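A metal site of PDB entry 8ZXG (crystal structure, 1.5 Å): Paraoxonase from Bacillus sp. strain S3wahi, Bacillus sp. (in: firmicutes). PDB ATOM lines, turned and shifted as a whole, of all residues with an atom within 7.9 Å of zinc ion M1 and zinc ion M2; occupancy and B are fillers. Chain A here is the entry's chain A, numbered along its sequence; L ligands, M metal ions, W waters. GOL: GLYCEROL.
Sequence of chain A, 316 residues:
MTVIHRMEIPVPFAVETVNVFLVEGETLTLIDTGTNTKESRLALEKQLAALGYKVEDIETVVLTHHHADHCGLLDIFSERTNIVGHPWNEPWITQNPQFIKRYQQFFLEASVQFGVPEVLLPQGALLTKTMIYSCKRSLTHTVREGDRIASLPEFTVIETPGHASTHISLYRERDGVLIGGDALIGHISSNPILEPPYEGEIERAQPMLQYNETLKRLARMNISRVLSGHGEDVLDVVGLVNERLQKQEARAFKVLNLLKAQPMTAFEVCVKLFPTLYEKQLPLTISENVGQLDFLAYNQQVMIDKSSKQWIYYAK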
ATOM      1  N   VAL A  11      -1.004  16.411  22.040  1.00  0.00           N
ATOM      2  CA  VAL A  11      -1.747  15.474  21.196  1.00  0.00           C
ATOM      3  C   VAL A  11      -2.315  16.247  20.025  1.00  0.00           C
ATOM      4  O   VAL A  11      -2.552  17.456  20.147  1.00  0.00           O
ATOM      5  CB  VAL A  11      -2.845  14.722  21.983  1.00  0.00           C
ATOM      6  CG1 VAL A  11      -2.206  13.871  23.076  1.00  0.00           C
ATOM      7  CG2 VAL A  11      -3.851  15.682  22.597  1.00  0.00           C
ATOM      8  N   PHE A  13      -5.106  16.592  18.704  1.00  0.00           N
ATOM      9  CA  PHE A  13      -6.538  16.717  18.865  1.00  0.00           C
ATOM     10  C   PHE A  13      -6.867  18.107  19.401  1.00  0.00           C
ATOM     11  O   PHE A  13      -5.976  18.804  19.885  1.00  0.00           O
ATOM     12  CB  PHE A  13      -7.049  15.665  19.855  1.00  0.00           C
ATOM     13  CG  PHE A  13      -6.735  14.216  19.483  1.00  0.00           C
ATOM     14  CD1 PHE A  13      -6.827  13.750  18.192  1.00  0.00           C
ATOM     15  CD2 PHE A  13      -6.444  13.312  20.465  1.00  0.00           C
ATOM     16  CE1 PHE A  13      -6.546  12.415  17.889  1.00  0.00           C
ATOM     17  CE2 PHE A  13      -6.182  11.973  20.171  1.00  0.00           C
ATOM     18  CZ  PHE A  13      -6.229  11.529  18.888  1.00  0.00           C
ATOM     19  N   VAL A  15      -8.174  19.118  22.047  1.00  0.00           N
ATOM     20  CA  VAL A  15      -7.877  19.293  23.465  1.00  0.00           C
ATOM     21  C   VAL A  15      -6.401  19.687  23.694  1.00  0.00           C
ATOM     22  O   VAL A  15      -6.023  20.124  24.796  1.00  0.00           O
ATOM     23  CB  VAL A  15      -8.261  18.011  24.207  1.00  0.00           C
ATOM     24  CG1 VAL A  15      -7.266  16.866  23.986  1.00  0.00           C
ATOM     25  CG2 VAL A  15      -8.427  18.274  25.691  1.00  0.00           C
ATOM     26  N   THR A  17      -3.584  18.871  24.691  1.00  0.00           N
ATOM     27  CA  THR A  17      -2.675  18.198  25.625  1.00  0.00           C
ATOM     28  C   THR A  17      -3.472  17.139  26.351  1.00  0.00           C
ATOM     29  O   THR A  17      -4.655  17.295  26.587  1.00  0.00           O
ATOM     30  CB  THR A  17      -1.993  19.110  26.647  1.00  0.00           C
ATOM     31  OG1 THR A  17      -2.948  19.661  27.502  1.00  0.00           O
ATOM     32  CG2 THR A  17      -1.264  20.200  25.899  1.00  0.00           C
ATOM     33  N   VAL A  18      -2.772  16.082  26.752  1.00  0.00           N
ATOM     34  CA  VAL A  18      -3.273  15.081  27.667  1.00  0.00           C
ATOM     35  C   VAL A  18      -2.384  15.133  28.909  1.00  0.00           C
ATOM     36  O   VAL A  18      -1.164  15.360  28.803  1.00  0.00           O
ATOM     37  CB  VAL A  18      -3.312  13.662  27.062  1.00  0.00           C
ATOM     38  CG1 VAL A  18      -1.933  13.113  26.721  1.00  0.00           C
ATOM     39  CG2 VAL A  18      -4.052  12.693  27.954  1.00  0.00           C
ATOM     40  N   ASN A  19      -2.991  14.937  30.077  1.00  0.00           N
ATOM     41  CA  ASN A  19      -2.243  14.857  31.311  1.00  0.00           C
ATOM     42  C   ASN A  19      -1.896  13.400  31.569  1.00  0.00           C
ATOM     43  O   ASN A  19      -2.808  12.554  31.592  1.00  0.00           O
ATOM     44  CB  ASN A  19      -3.033  15.369  32.488  1.00  0.00           C
ATOM     45  CG  ASN A  19      -3.397  16.825  32.370  1.00  0.00           C
ATOM     46  OD1 ASN A  19      -2.614  17.632  31.824  1.00  0.00           O
ATOM     47  ND2 ASN A  19      -4.560  17.172  32.945  1.00  0.00           N
ATOM     48  N   ASP A  32      -1.368   6.703  31.876  1.00  0.00           N
ATOM     49  CA  ASP A  32      -1.647   7.248  30.544  1.00  0.00           C
ATOM     50  C   ASP A  32      -0.365   7.678  29.838  1.00  0.00           C
ATOM     51  O   ASP A  32       0.673   7.852  30.482  1.00  0.00           O
ATOM     52  CB  ASP A  32      -2.777   8.262  30.605  1.00  0.00           C
ATOM     53  CG  ASP A  32      -4.116   7.680  30.985  1.00  0.00           C
ATOM     54  OD1 ASP A  32      -4.250   6.405  30.896  1.00  0.00           O
ATOM     55  OD2 ASP A  32      -5.037   8.454  31.305  1.00  0.00           O
ATOM     56  N   THR A  64      -6.152   4.573  31.894  1.00  0.00           N
ATOM     57  CA  THR A  64      -7.492   4.893  32.314  1.00  0.00           C
ATOM     58  C   THR A  64      -8.526   4.409  31.308  1.00  0.00           C
ATOM     59  O   THR A  64      -9.646   4.062  31.696  1.00  0.00           O
ATOM     60  CB  THR A  64      -7.699   6.392  32.602  1.00  0.00           C
ATOM     61  OG1 THR A  64      -7.433   7.149  31.397  1.00  0.00           O
ATOM     62  CG2 THR A  64      -6.820   6.870  33.732  1.00  0.00           C
ATOM     63  N   HIS A  65      -8.171   4.417  30.010  1.00  0.00           N
ATOM     64  CA  HIS A  65      -9.061   3.945  28.953  1.00  0.00           C
ATOM     65  C   HIS A  65      -8.301   3.825  27.632  1.00  0.00           C
ATOM     66  O   HIS A  65      -7.142   4.180  27.551  1.00  0.00           O
ATOM     67  CB  HIS A  65     -10.304   4.852  28.859  1.00  0.00           C
ATOM     68  CG  HIS A  65     -10.094   6.276  28.471  1.00  0.00           C
ATOM     69  ND1 HIS A  65      -9.301   7.154  29.172  1.00  0.00           N
ATOM     70  CD2 HIS A  65     -10.647   6.994  27.445  1.00  0.00           C
ATOM     71  CE1 HIS A  65      -9.418   8.362  28.634  1.00  0.00           C
ATOM     72  NE2 HIS A  65     -10.237   8.282  27.598  1.00  0.00           N
ATOM     73  N   HIS A  66      -9.005   3.319  26.592  1.00  0.00           N
ATOM     74  CA  HIS A  66      -8.358   2.919  25.349  1.00  0.00           C
ATOM     75  C   HIS A  66      -8.183   4.057  24.333  1.00  0.00           C
ATOM     76  O   HIS A  66      -7.584   3.848  23.289  1.00  0.00           O
ATOM     77  CB  HIS A  66      -9.202   1.846  24.679  1.00  0.00           C
ATOM     78  CG  HIS A  66     -10.502   2.340  24.105  1.00  0.00           C
ATOM     79  ND1 HIS A  66     -11.680   2.298  24.794  1.00  0.00           N
ATOM     80  CD2 HIS A  66     -10.799   2.804  22.869  1.00  0.00           C
ATOM     81  CE1 HIS A  66     -12.660   2.759  24.047  1.00  0.00           C
ATOM     82  NE2 HIS A  66     -12.134   3.078  22.862  1.00  0.00           N
ATOM     83  N   HIS A  67      -8.701   5.255  24.651  1.00  0.00           N
ATOM     84  CA  HIS A  67      -8.578   6.337  23.685  1.00  0.00           C
ATOM     85  C   HIS A  67      -7.089   6.602  23.402  1.00  0.00           C
ATOM     86  O   HIS A  67      -6.249   6.478  24.263  1.00  0.00           O
ATOM     87  CB  HIS A  67      -9.295   7.590  24.171  1.00  0.00           C
ATOM     88  CG  HIS A  67     -10.775   7.475  24.240  1.00  0.00           C
ATOM     89  ND1 HIS A  67     -11.603   8.391  24.830  1.00  0.00           N
ATOM     90  CD2 HIS A  67     -11.595   6.514  23.711  1.00  0.00           C
ATOM     91  CE1 HIS A  67     -12.856   8.009  24.658  1.00  0.00           C
ATOM     92  NE2 HIS A  67     -12.882   6.854  23.978  1.00  0.00           N
ATOM     93  N   ALA A  68      -6.783   6.929  22.150  1.00  0.00           N
ATOM     94  CA  ALA A  68      -5.414   6.991  21.663  1.00  0.00           C
ATOM     95  C   ALA A  68      -4.519   7.969  22.413  1.00  0.00           C
ATOM     96  O   ALA A  68      -3.302   7.730  22.521  1.00  0.00           O
ATOM     97  CB  ALA A  68      -5.407   7.349  20.185  1.00  0.00           C
ATOM     98  N   ASP A  69      -5.124   9.053  22.941  1.00  0.00           N
ATOM     99  CA  ASP A  69      -4.344   9.998  23.721  1.00  0.00           C
ATOM    100  C   ASP A  69      -3.847   9.418  25.064  1.00  0.00           C
ATOM    101  O   ASP A  69      -2.919   9.975  25.666  1.00  0.00           O
ATOM    102  CB  ASP A  69      -5.076  11.318  23.884  1.00  0.00           C
ATOM    103  CG  ASP A  69      -6.559  11.261  24.256  1.00  0.00           C
ATOM    104  OD1 ASP A  69      -7.441  10.388  23.868  1.00  0.00           O
ATOM    105  OD2 ASP A  69      -6.977  12.137  25.080  1.00  0.00           O
ATOM    106  N   HIS A  70      -4.448   8.305  25.501  1.00  0.00           N
ATOM    107  CA  HIS A  70      -4.100   7.689  26.773  1.00  0.00           C
ATOM    108  C   HIS A  70      -3.238   6.424  26.638  1.00  0.00           C
ATOM    109  O   HIS A  70      -2.558   6.083  27.579  1.00  0.00           O
ATOM    110  CB  HIS A  70      -5.358   7.478  27.599  1.00  0.00           C
ATOM    111  CG  HIS A  70      -6.112   8.752  27.832  1.00  0.00           C
ATOM    112  ND1 HIS A  70      -6.015   9.494  28.977  1.00  0.00           N
ATOM    113  CD2 HIS A  70      -6.876   9.448  26.994  1.00  0.00           C
ATOM    114  CE1 HIS A  70      -6.708  10.610  28.847  1.00  0.00           C
ATOM    115  NE2 HIS A  70      -7.255  10.594  27.635  1.00  0.00           N
ATOM    116  N   HIS A 163     -17.762   7.651  29.412  1.00  0.00           N
ATOM    117  CA  HIS A 163     -16.877   8.275  28.463  1.00  0.00           C
ATOM    118  C   HIS A 163     -16.345   7.233  27.483  1.00  0.00           C
ATOM    119  O   HIS A 163     -16.219   7.501  26.287  1.00  0.00           O
ATOM    120  CB  HIS A 163     -15.720   8.969  29.180  1.00  0.00           C
ATOM    121  CG  HIS A 163     -14.722   9.555  28.252  1.00  0.00           C
ATOM    122  ND1 HIS A 163     -14.935  10.719  27.555  1.00  0.00           N
ATOM    123  CD2 HIS A 163     -13.494   9.143  27.909  1.00  0.00           C
ATOM    124  CE1 HIS A 163     -13.855  11.004  26.817  1.00  0.00           C
ATOM    125  NE2 HIS A 163     -12.963  10.072  27.039  1.00  0.00           N
ATOM    126  N   ALA A 164     -15.999   6.073  27.999  1.00  0.00           N
ATOM    127  CA  ALA A 164     -15.585   4.909  27.217  1.00  0.00           C
ATOM    128  C   ALA A 164     -15.952   3.670  28.009  1.00  0.00           C
ATOM    129  O   ALA A 164     -16.007   3.713  29.228  1.00  0.00           O
ATOM    130  CB  ALA A 164     -14.096   4.932  26.969  1.00  0.00           C
ATOM    131  N   HIS A 167     -13.330   2.576  30.644  1.00  0.00           N
ATOM    132  CA  HIS A 167     -12.870   3.659  31.521  1.00  0.00           C
ATOM    133  C   HIS A 167     -12.810   3.242  32.990  1.00  0.00           C
ATOM    134  O   HIS A 167     -13.798   2.792  33.547  1.00  0.00           O
ATOM    135  CB  HIS A 167     -13.729   4.917  31.311  1.00  0.00           C
ATOM    136  CG  HIS A 167     -13.026   6.137  31.716  1.00  0.00           C
ATOM    137  ND1 HIS A 167     -12.879   6.523  33.037  1.00  0.00           N
ATOM    138  CD2 HIS A 167     -12.253   6.980  30.979  1.00  0.00           C
ATOM    139  CE1 HIS A 167     -12.108   7.595  33.066  1.00  0.00           C
ATOM    140  NE2 HIS A 167     -11.716   7.893  31.827  1.00  0.00           N
ATOM    141  N   GLY A 181      -8.881  10.107  34.897  1.00  0.00           N
ATOM    142  CA  GLY A 181      -9.041   9.934  33.464  1.00  0.00           C
ATOM    143  C   GLY A 181      -9.928  11.019  32.885  1.00  0.00           C
ATOM    144  O   GLY A 181      -9.885  12.170  33.340  1.00  0.00           O
ATOM    145  N   ASP A 182     -10.769  10.619  31.913  1.00  0.00           N
ATOM    146  CA  ASP A 182     -11.665  11.528  31.243  1.00  0.00           C
ATOM    147  C   ASP A 182     -13.102  11.476  31.760  1.00  0.00           C
ATOM    148  O   ASP A 182     -14.007  11.999  31.129  1.00  0.00           O
ATOM    149  CB  ASP A 182     -11.598  11.323  29.744  1.00  0.00           C
ATOM    150  CG  ASP A 182     -10.289  11.711  29.049  1.00  0.00           C
ATOM    151  OD1 ASP A 182      -9.367  12.188  29.813  1.00  0.00           O
ATOM    152  OD2 ASP A 182     -10.183  11.479  27.785  1.00  0.00           O
ATOM    153  N   ALA A 183     -13.323  10.874  32.930  1.00  0.00           N
ATOM    154  CA  ALA A 183     -14.666  10.748  33.458  1.00  0.00           C
ATOM    155  C   ALA A 183     -15.269  12.108  33.795  1.00  0.00           C
ATOM    156  O   ALA A 183     -16.458  12.295  33.549  1.00  0.00           O
ATOM    157  CB  ALA A 183     -14.706   9.855  34.652  1.00  0.00           C
ATOM    158  N   ILE A 185     -14.000  16.157  33.354  1.00  0.00           N
ATOM    159  CA  ILE A 185     -13.059  17.169  32.906  1.00  0.00           C
ATOM    160  C   ILE A 185     -13.645  18.541  33.230  1.00  0.00           C
ATOM    161  O   ILE A 185     -14.826  18.789  32.981  1.00  0.00           O
ATOM    162  CB  ILE A 185     -12.783  16.979  31.407  1.00  0.00           C
ATOM    163  CG1 ILE A 185     -12.184  15.608  31.151  1.00  0.00           C
ATOM    164  CG2 ILE A 185     -11.881  18.083  30.862  1.00  0.00           C
ATOM    165  CD1 ILE A 185     -12.135  15.260  29.687  1.00  0.00           C
ATOM    166  N   SER A 190     -17.333  15.416  28.811  1.00  0.00           N
ATOM    167  CA  SER A 190     -16.582  14.243  28.394  1.00  0.00           C
ATOM    168  C   SER A 190     -17.568  13.145  28.020  1.00  0.00           C
ATOM    169  O   SER A 190     -17.365  11.978  28.368  1.00  0.00           O
ATOM    170  CB  SER A 190     -15.624  13.758  29.486  1.00  0.00           C
ATOM    171  OG  SER A 190     -16.135  13.954  30.777  1.00  0.00           O
ATOM    172  N   ASN A 191     -18.640  13.541  27.288  1.00  0.00           N
ATOM    173  CA  ASN A 191     -19.796  12.693  27.094  1.00  0.00           C
ATOM    174  C   ASN A 191     -19.377  11.438  26.339  1.00  0.00           C
ATOM    175  O   ASN A 191     -18.352  11.435  25.713  1.00  0.00           O
ATOM    176  CB  ASN A 191     -20.855  13.433  26.308  1.00  0.00           C
ATOM    177  CG  ASN A 191     -21.675  14.328  27.224  1.00  0.00           C
ATOM    178  OD1 ASN A 191     -21.475  14.326  28.451  1.00  0.00           O
ATOM    179  ND2 ASN A 191     -22.606  15.058  26.655  1.00  0.00           N
ATOM    180  N   ILE A 193     -18.222   8.711  23.937  1.00  0.00           N
ATOM    181  CA  ILE A 193     -17.671   8.572  22.607  1.00  0.00           C
ATOM    182  C   ILE A 193     -18.155   7.246  22.012  1.00  0.00           C
ATOM    183  O   ILE A 193     -17.917   6.202  22.619  1.00  0.00           O
ATOM    184  CB  ILE A 193     -16.127   8.620  22.693  1.00  0.00           C
ATOM    185  CG1 ILE A 193     -15.615   9.911  23.415  1.00  0.00           C
ATOM    186  CG2 ILE A 193     -15.495   8.410  21.316  1.00  0.00           C
ATOM    187  CD1 ILE A 193     -16.145  11.177  22.809  1.00  0.00           C
ATOM    188  N   GLY A 229      -7.643  13.767  33.052  1.00  0.00           N
ATOM    189  CA  GLY A 229      -6.903  13.435  31.849  1.00  0.00           C
ATOM    190  C   GLY A 229      -6.604  14.651  30.991  1.00  0.00           C
ATOM    191  O   GLY A 229      -5.687  14.610  30.203  1.00  0.00           O
ATOM    192  N   HIS A 230      -7.420  15.721  31.148  1.00  0.00           N
ATOM    193  CA  HIS A 230      -7.225  16.939  30.407  1.00  0.00           C
ATOM    194  C   HIS A 230      -7.544  18.140  31.263  1.00  0.00           C
ATOM    195  O   HIS A 230      -8.491  18.118  32.018  1.00  0.00           O
ATOM    196  CB  HIS A 230      -8.074  16.972  29.135  1.00  0.00           C
ATOM    197  CG  HIS A 230      -7.883  15.794  28.242  1.00  0.00           C
ATOM    198  ND1 HIS A 230      -6.826  15.718  27.356  1.00  0.00           N
ATOM    199  CD2 HIS A 230      -8.553  14.650  28.148  1.00  0.00           C
ATOM    200  CE1 HIS A 230      -6.885  14.512  26.747  1.00  0.00           C
ATOM    201  NE2 HIS A 230      -7.923  13.858  27.240  1.00  0.00           N
HETATM  202  C1  GOL L   1     -13.429  14.124  24.456  1.00  0.00           C
HETATM  203  O1  GOL L   1     -13.868  15.287  23.752  1.00  0.00           O
HETATM  204  C2  GOL L   1     -12.006  14.262  24.937  1.00  0.00           C
HETATM  205  O2  GOL L   1     -11.234  15.069  24.051  1.00  0.00           O
HETATM  206  C3  GOL L   1     -11.286  12.949  25.152  1.00  0.00           C
HETATM  207  O3  GOL L   1      -9.900  13.163  25.401  1.00  0.00           O
HETATM  208 ZN    ZN M   1      -8.550  11.964  26.590  1.00  0.00          ZN
HETATM  209 ZN    ZN M   2     -11.005   9.904  26.278  1.00  0.00          ZN
HETATM  210 MG    MG M   3     -15.198   5.396  23.347  1.00  0.00          MG
HETATM  211 MG    MG M   4     -13.550   4.830  21.052  1.00  0.00          MG
HETATM  212  O   HOH W   1      -9.122  10.480  25.308  1.00  0.00           O
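The backbone NH of Asp 182 is in hydrogen-bond range of a ring nitrogen (NE2) of His 167, 2.9 Å away.
The backbone carbonyl oxygen (O) of Asp 182 sits close to the side-chain hydroxyl (OG) of Ser 190, 2.9 Å away.
The backbone carbonyl oxygen of Thr 17 sits at hydrogen-bond distance from a ring nitrogen (ND1) of His 230, at 2.8 Å.
The backbone carbonyl oxygen (O) of His 163 sits at hydrogen-bond distance from the backbone NH (N) of Ile 193 (3.3 Å).
A ring nitrogen (ND1) of His 163 lies within hydrogen-bond range of the backbone carbonyl oxygen (O) of Ser 190 (2.9 Å).
A ring nitrogen (ND1) of His 70 sits at hydrogen-bond distance from the side-chain carboxylate of Asp 32 (2.7 Å).
A ring nitrogen (ND1) of His 65 is in hydrogen-bond range of the side-chain hydroxyl of Thr 64, 2.9 Å away.
Of the 26 residues printed, 4 come within 4 Å of zinc ion M1.
Four residues have an atom within 4 Å of zinc ion M2: His 65, His 67, His 163 and Asp 182.
The nearest printed residue that does not touch zinc ion M2 is His 70 (4.05 Å).
Water W1 binds zinc ion M1 (2.0 Å).
The side-chain carboxylate (OD2) of Asp 182 is bound to zinc ion M1.
Zinc ion M1 is bound by a ring nitrogen (NE2) of His 230 (2.1 Å).
A ring nitrogen (NE2) of His 70 is bound to zinc ion M1, at 2.2 Å.
O3 of the ligand is bound to zinc ion M1, at 2.2 Å.
The side-chain carboxylate (OD2) of Asp 69 binds zinc ion M1 (2.2 Å).
Zinc ion M2 is bound by a ring nitrogen (NE2) of His 163, a ring nitrogen (ND1) of His 67, water W1, a ring nitrogen (NE2) of His 65 and the side-chain carboxylate (OD2) of Asp 182.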
